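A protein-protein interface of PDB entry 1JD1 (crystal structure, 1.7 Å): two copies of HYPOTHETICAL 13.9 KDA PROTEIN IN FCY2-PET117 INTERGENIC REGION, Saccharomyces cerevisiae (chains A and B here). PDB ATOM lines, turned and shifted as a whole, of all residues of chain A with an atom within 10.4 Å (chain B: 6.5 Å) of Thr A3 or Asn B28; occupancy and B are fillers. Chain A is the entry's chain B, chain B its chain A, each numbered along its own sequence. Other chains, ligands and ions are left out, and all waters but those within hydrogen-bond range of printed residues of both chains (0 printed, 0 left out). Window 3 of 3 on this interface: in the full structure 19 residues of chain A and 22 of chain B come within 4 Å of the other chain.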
ATOM      1  N   THR A   3     -24.000  11.242  13.192  1.00  0.00           N
ATOM      2  CA  THR A   3     -23.152  10.284  13.972  1.00  0.00           C
ATOM      3  C   THR A   3     -23.990   9.152  14.562  1.00  0.00           C
ATOM      4  O   THR A   3     -24.837   9.384  15.423  1.00  0.00           O
ATOM      5  CB  THR A   3     -22.430  11.004  15.119  1.00  0.00           C
ATOM      6  OG1 THR A   3     -21.608  12.042  14.577  1.00  0.00           O
ATOM      7  CG2 THR A   3     -21.557  10.032  15.899  1.00  0.00           C
ATOM      8  N   THR A   4     -23.744   7.929  14.105  1.00  0.00           N
ATOM      9  CA  THR A   4     -24.488   6.775  14.592  1.00  0.00           C
ATOM     10  C   THR A   4     -23.635   5.882  15.500  1.00  0.00           C
ATOM     11  O   THR A   4     -22.490   5.577  15.175  1.00  0.00           O
ATOM     12  CB  THR A   4     -25.030   5.937  13.413  1.00  0.00           C
ATOM     13  OG1 THR A   4     -23.944   5.317  12.715  1.00  0.00           O
ATOM     14  CG2 THR A   4     -25.781   6.830  12.435  1.00  0.00           C
ATOM     15  N   LEU A   5     -24.187   5.492  16.648  1.00  0.00           N
ATOM     16  CA  LEU A   5     -23.478   4.615  17.583  1.00  0.00           C
ATOM     17  C   LEU A   5     -24.103   3.232  17.537  1.00  0.00           C
ATOM     18  O   LEU A   5     -25.312   3.086  17.756  1.00  0.00           O
ATOM     19  CB  LEU A   5     -23.568   5.139  19.020  1.00  0.00           C
ATOM     20  CG  LEU A   5     -23.063   6.551  19.319  1.00  0.00           C
ATOM     21  CD1 LEU A   5     -22.894   6.704  20.828  1.00  0.00           C
ATOM     22  CD2 LEU A   5     -21.729   6.793  18.629  1.00  0.00           C
ATOM     23  N   THR A   6     -23.300   2.213  17.253  1.00  0.00           N
ATOM     24  CA  THR A   6     -23.832   0.858  17.199  1.00  0.00           C
ATOM     25  C   THR A   6     -23.022  -0.121  18.056  1.00  0.00           C
ATOM     26  O   THR A   6     -21.850  -0.415  17.772  1.00  0.00           O
ATOM     27  CB  THR A   6     -23.948   0.366  15.710  1.00  0.00           C
ATOM     28  OG1 THR A   6     -24.247  -1.036  15.669  1.00  0.00           O
ATOM     29  CG2 THR A   6     -22.679   0.605  14.968  1.00  0.00           C
ATOM     30  N   MET A  24     -17.889  -0.860  20.228  1.00  0.00           N
ATOM     31  CA  MET A  24     -18.866   0.189  19.949  1.00  0.00           C
ATOM     32  C   MET A  24     -18.440   0.851  18.658  1.00  0.00           C
ATOM     33  O   MET A  24     -17.298   1.301  18.541  1.00  0.00           O
ATOM     34  CB  MET A  24     -18.894   1.227  21.082  1.00  0.00           C
ATOM     35  CG  MET A  24     -19.907   2.378  20.903  1.00  0.00           C
ATOM     36  SD  MET A  24     -21.700   1.872  20.881  1.00  0.00           S
ATOM     37  CE  MET A  24     -21.974   1.497  22.506  1.00  0.00           C
ATOM     38  N   LYS A  25     -19.340   0.900  17.676  1.00  0.00           N
ATOM     39  CA  LYS A  25     -19.003   1.558  16.420  1.00  0.00           C
ATOM     40  C   LYS A  25     -19.537   2.982  16.487  1.00  0.00           C
ATOM     41  O   LYS A  25     -20.632   3.220  16.997  1.00  0.00           O
ATOM     42  CB  LYS A  25     -19.657   0.884  15.209  1.00  0.00           C
ATOM     43  CG  LYS A  25     -19.502  -0.613  15.078  1.00  0.00           C
ATOM     44  CD  LYS A  25     -20.194  -1.091  13.791  1.00  0.00           C
ATOM     45  CE  LYS A  25     -20.273  -2.598  13.714  1.00  0.00           C
ATOM     46  NZ  LYS A  25     -20.823  -3.011  12.381  1.00  0.00           N
ATOM     47  N   VAL A  26     -18.735   3.928  16.023  1.00  0.00           N
ATOM     48  CA  VAL A  26     -19.144   5.321  15.937  1.00  0.00           C
ATOM     49  C   VAL A  26     -18.880   5.563  14.456  1.00  0.00           C
ATOM     50  O   VAL A  26     -17.729   5.648  14.000  1.00  0.00           O
ATOM     51  CB  VAL A  26     -18.304   6.259  16.848  1.00  0.00           C
ATOM     52  CG1 VAL A  26     -16.820   6.025  16.647  1.00  0.00           C
ATOM     53  CG2 VAL A  26     -18.664   7.707  16.551  1.00  0.00           C
ATOM     54  N   ASN A  27     -19.970   5.635  13.702  1.00  0.00           N
ATOM     55  CA  ASN A  27     -19.891   5.760  12.257  1.00  0.00           C
ATOM     56  C   ASN A  27     -19.068   4.558  11.801  1.00  0.00           C
ATOM     57  O   ASN A  27     -19.432   3.434  12.123  1.00  0.00           O
ATOM     58  CB  ASN A  27     -19.285   7.107  11.834  1.00  0.00           C
ATOM     59  CG  ASN A  27     -20.323   8.236  11.860  1.00  0.00           C
ATOM     60  OD1 ASN A  27     -20.022   9.398  11.576  1.00  0.00           O
ATOM     61  ND2 ASN A  27     -21.558   7.884  12.208  1.00  0.00           N
ATOM     62  N   ASN A  28     -17.954   4.764  11.117  1.00  0.00           N
ATOM     63  CA  ASN A  28     -17.168   3.632  10.620  1.00  0.00           C
ATOM     64  C   ASN A  28     -15.960   3.227  11.471  1.00  0.00           C
ATOM     65  O   ASN A  28     -15.161   2.380  11.054  1.00  0.00           O
ATOM     66  CB  ASN A  28     -16.680   3.950   9.210  1.00  0.00           C
ATOM     67  CG  ASN A  28     -15.494   4.877   9.218  1.00  0.00           C
ATOM     68  OD1 ASN A  28     -15.507   5.926   9.882  1.00  0.00           O
ATOM     69  ND2 ASN A  28     -14.448   4.501   8.488  1.00  0.00           N
ATOM     70  N   LEU A  29     -15.823   3.835  12.643  1.00  0.00           N
ATOM     71  CA  LEU A  29     -14.701   3.553  13.536  1.00  0.00           C
ATOM     72  C   LEU A  29     -15.206   2.628  14.639  1.00  0.00           C
ATOM     73  O   LEU A  29     -16.251   2.885  15.249  1.00  0.00           O
ATOM     74  CB  LEU A  29     -14.195   4.872  14.122  1.00  0.00           C
ATOM     75  CG  LEU A  29     -12.709   5.063  14.416  1.00  0.00           C
ATOM     76  CD1 LEU A  29     -11.866   4.742  13.192  1.00  0.00           C
ATOM     77  CD2 LEU A  29     -12.491   6.509  14.828  1.00  0.00           C
ATOM     78  N   PHE A  31     -14.417   0.832  18.286  1.00  0.00           N
ATOM     79  CA  PHE A  31     -13.597   0.807  19.492  1.00  0.00           C
ATOM     80  C   PHE A  31     -13.885  -0.522  20.209  1.00  0.00           C
ATOM     81  O   PHE A  31     -15.018  -0.786  20.657  1.00  0.00           O
ATOM     82  CB  PHE A  31     -13.922   2.006  20.405  1.00  0.00           C
ATOM     83  CG  PHE A  31     -13.431   3.325  19.870  1.00  0.00           C
ATOM     84  CD1 PHE A  31     -14.096   3.956  18.815  1.00  0.00           C
ATOM     85  CD2 PHE A  31     -12.258   3.901  20.364  1.00  0.00           C
ATOM     86  CE1 PHE A  31     -13.594   5.135  18.260  1.00  0.00           C
ATOM     87  CE2 PHE A  31     -11.753   5.080  19.814  1.00  0.00           C
ATOM     88  CZ  PHE A  31     -12.416   5.695  18.764  1.00  0.00           C
ATOM     89  N   THR B   4     -12.214  20.382  12.187  1.00  0.00           N
ATOM     90  CA  THR B   4     -12.228  21.462  13.163  1.00  0.00           C
ATOM     91  C   THR B   4     -11.912  20.900  14.545  1.00  0.00           C
ATOM     92  O   THR B   4     -12.493  19.891  14.959  1.00  0.00           O
ATOM     93  CB  THR B   4     -13.602  22.156  13.199  1.00  0.00           C
ATOM     94  OG1 THR B   4     -14.621  21.186  13.484  1.00  0.00           O
ATOM     95  CG2 THR B   4     -13.904  22.794  11.849  1.00  0.00           C
ATOM     96  N   LYS B  25     -12.710  18.427  20.890  1.00  0.00           N
ATOM     97  CA  LYS B  25     -13.599  17.892  19.881  1.00  0.00           C
ATOM     98  C   LYS B  25     -12.915  17.963  18.525  1.00  0.00           C
ATOM     99  O   LYS B  25     -12.308  18.980  18.180  1.00  0.00           O
ATOM    100  CB  LYS B  25     -14.925  18.671  19.882  1.00  0.00           C
ATOM    101  CG  LYS B  25     -15.569  18.710  21.262  1.00  0.00           C
ATOM    102  CD  LYS B  25     -17.048  19.049  21.223  1.00  0.00           C
ATOM    103  CE  LYS B  25     -17.300  20.485  20.806  1.00  0.00           C
ATOM    104  NZ  LYS B  25     -18.762  20.798  20.858  1.00  0.00           N
ATOM    105  N   VAL B  26     -12.947  16.855  17.787  1.00  0.00           N
ATOM    106  CA  VAL B  26     -12.382  16.808  16.446  1.00  0.00           C
ATOM    107  C   VAL B  26     -13.583  16.393  15.608  1.00  0.00           C
ATOM    108  O   VAL B  26     -13.984  15.223  15.572  1.00  0.00           O
ATOM    109  CB  VAL B  26     -11.195  15.805  16.335  1.00  0.00           C
ATOM    110  CG1 VAL B  26     -11.571  14.447  16.905  1.00  0.00           C
ATOM    111  CG2 VAL B  26     -10.760  15.690  14.876  1.00  0.00           C
ATOM    112  N   ASN B  27     -14.169  17.393  14.952  1.00  0.00           N
ATOM    113  CA  ASN B  27     -15.382  17.213  14.170  1.00  0.00           C
ATOM    114  C   ASN B  27     -16.460  16.674  15.102  1.00  0.00           C
ATOM    115  O   ASN B  27     -16.800  17.344  16.070  1.00  0.00           O
ATOM    116  CB  ASN B  27     -15.136  16.298  12.971  1.00  0.00           C
ATOM    117  CG  ASN B  27     -14.464  17.033  11.822  1.00  0.00           C
ATOM    118  OD1 ASN B  27     -14.120  16.445  10.792  1.00  0.00           O
ATOM    119  ND2 ASN B  27     -14.270  18.339  12.001  1.00  0.00           N
ATOM    120  N   ASN B  28     -16.984  15.480  14.850  1.00  0.00           N
ATOM    121  CA  ASN B  28     -18.047  14.954  15.702  1.00  0.00           C
ATOM    122  C   ASN B  28     -17.592  14.076  16.875  1.00  0.00           C
ATOM    123  O   ASN B  28     -18.423  13.632  17.670  1.00  0.00           O
ATOM    124  CB  ASN B  28     -19.057  14.194  14.846  1.00  0.00           C
ATOM    125  N   LEU B  29     -16.293  13.812  16.983  1.00  0.00           N
ATOM    126  CA  LEU B  29     -15.797  12.985  18.082  1.00  0.00           C
ATOM    127  C   LEU B  29     -15.265  13.880  19.180  1.00  0.00           C
ATOM    128  O   LEU B  29     -14.737  14.955  18.914  1.00  0.00           O
ATOM    129  CB  LEU B  29     -14.660  12.062  17.639  1.00  0.00           C
ATOM    130  CG  LEU B  29     -14.890  10.926  16.653  1.00  0.00           C
ATOM    131  CD1 LEU B  29     -13.606  10.090  16.587  1.00  0.00           C
ATOM    132  CD2 LEU B  29     -16.072  10.069  17.090  1.00  0.00           C
ATOM    133  N   ILE B  30     -15.396  13.420  20.415  1.00  0.00           N
ATOM    134  CA  ILE B  30     -14.936  14.175  21.565  1.00  0.00           C
ATOM    135  C   ILE B  30     -13.988  13.323  22.411  1.00  0.00           C
ATOM    136  O   ILE B  30     -14.369  12.245  22.870  1.00  0.00           O
ATOM    137  CB  ILE B  30     -16.110  14.565  22.483  1.00  0.00           C
ATOM    138  CG1 ILE B  30     -17.180  15.288  21.675  1.00  0.00           C
ATOM    139  CG2 ILE B  30     -15.609  15.451  23.629  1.00  0.00           C
ATOM    140  CD1 ILE B  30     -18.484  15.464  22.420  1.00  0.00           C
ATOM    141  N   ARG B  73     -24.067   8.854  24.865  1.00  0.00           N
ATOM    142  CA  ARG B  73     -23.352   9.046  23.599  1.00  0.00           C
ATOM    143  C   ARG B  73     -21.860   8.703  23.777  1.00  0.00           C
ATOM    144  O   ARG B  73     -21.037   9.006  22.910  1.00  0.00           O
ATOM    145  CB  ARG B  73     -23.475  10.494  23.104  1.00  0.00           C
ATOM    146  CG  ARG B  73     -24.907  10.962  22.798  1.00  0.00           C
ATOM    147  CD  ARG B  73     -25.011  11.598  21.423  1.00  0.00           C
ATOM    148  NE  ARG B  73     -24.942  10.594  20.362  1.00  0.00           N
ATOM    149  CZ  ARG B  73     -24.895  10.870  19.060  1.00  0.00           C
ATOM    150  NH1 ARG B  73     -24.904  12.127  18.636  1.00  0.00           N
ATOM    151  NH2 ARG B  73     -24.840   9.880  18.176  1.00  0.00           N
ATOM    152  N   ALA B 125     -16.410  10.248  23.202  1.00  0.00           N
ATOM    153  CA  ALA B 125     -17.860  10.323  23.033  1.00  0.00           C
ATOM    154  C   ALA B 125     -18.225  10.970  21.702  1.00  0.00           C
ATOM    155  O   ALA B 125     -17.383  11.561  21.038  1.00  0.00           O
ATOM    156  CB  ALA B 125     -18.452  11.136  24.195  1.00  0.00           C
ATOM    157  N   ALA B 126     -19.490  10.842  21.315  1.00  0.00           N
ATOM    158  CA  ALA B 126     -19.983  11.427  20.077  1.00  0.00           C
ATOM    159  C   ALA B 126     -20.738  12.704  20.410  1.00  0.00           C
ATOM    160  O   ALA B 126     -21.474  12.756  21.389  1.00  0.00           O
ATOM    161  CB  ALA B 126     -20.924  10.446  19.382  1.00  0.00           C
ATOM    162  N   GLU B 127     -20.558  13.748  19.618  1.00  0.00           N
ATOM    163  CA  GLU B 127     -21.310  14.964  19.890  1.00  0.00           C
ATOM    164  C   GLU B 127     -22.758  14.710  19.405  1.00  0.00           C
ATOM    165  O   GLU B 127     -22.972  13.847  18.556  1.00  0.00           O
ATOM    166  CB  GLU B 127     -20.674  16.132  19.134  1.00  0.00           C
ATOM    167  CG  GLU B 127     -21.412  17.424  19.307  1.00  0.00           C
ATOM    168  CD  GLU B 127     -20.672  18.609  18.732  1.00  0.00           C
ATOM    169  OE1 GLU B 127     -20.044  18.469  17.660  1.00  0.00           O
ATOM    170  OE2 GLU B 127     -20.734  19.690  19.356  1.00  0.00           O
ATOM    171  N   ARG B 128     -23.725  15.449  19.967  1.00  0.00           N
ATOM    172  CA  ARG B 128     -25.156  15.362  19.622  1.00  0.00           C
ATOM    173  C   ARG B 128     -25.404  15.879  18.190  1.00  0.00           C
ATOM    174  O   ARG B 128     -24.517  16.493  17.598  1.00  0.00           O
ATOM    175  CB  ARG B 128     -26.026  16.204  20.658  1.00  0.00           C
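Val A26 touches Leu B29, but with the chains exchanged Leu A29 does not touch Val B26 (8.3 Å). Positions printed for both chains: 4, 25, 26, 27, 28 and 29.
O of Thr A3 sits at hydrogen-bond distance from NH2 of Arg B73 (2.8 Å).
N of Glu B127 is in hydrogen-bond range of O of Asn B28 (2.9 Å). The backbone carbonyl oxygen (O) of Arg B73 sits at hydrogen-bond distance from the backbone NH (N) of Ala B126 (2.9 Å). The guanidinium group (NH1) of Arg B73 lies within hydrogen-bond range of the backbone carbonyl oxygen (O) of Glu B127 (2.6 Å).
Asn B28 touches Thr A3 (CB to OG1, 3.3 Å). CG2 of Thr A3 touches CB of Ala B126, at 3.6 Å. O of Arg B73 touches CD1 of Leu A5, 3.6 Å away. Ala B126 touches Leu A5. Val A26 touches Leu B29.
Of chain B, only Asn B28 (3.3 Å), Arg B73 (2.8 Å) and Ala B126 (3.6 Å) come within 4 Å of Thr A3. Of the printed residues of chain B, Leu A5 touches Arg B73 (3.6 Å) and Ala B126 (3.8 Å). Leu A29 touches none of the printed residues of chain B. Phe A31 touches none of the printed residues of chain B. No residue of chain A comes within 4 Å of Asn B27. Leu B29 touches one residue of chain A. Of the printed residues of chain A, Arg B73 touches Thr A3 and Leu A5.
Of the 11 printed residues of chain A, 3 touch a printed residue of chain B. Printed residues of chain A that touch a printed residue of chain B: Thr A3, Leu A5 and Val A26. Among the printed residues, 6 pairs touch across the chains. Among the printed residues, no Asp or Glu carboxylate lies within 4 Å of a Lys or Arg side-chain nitrogen of the other chain.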
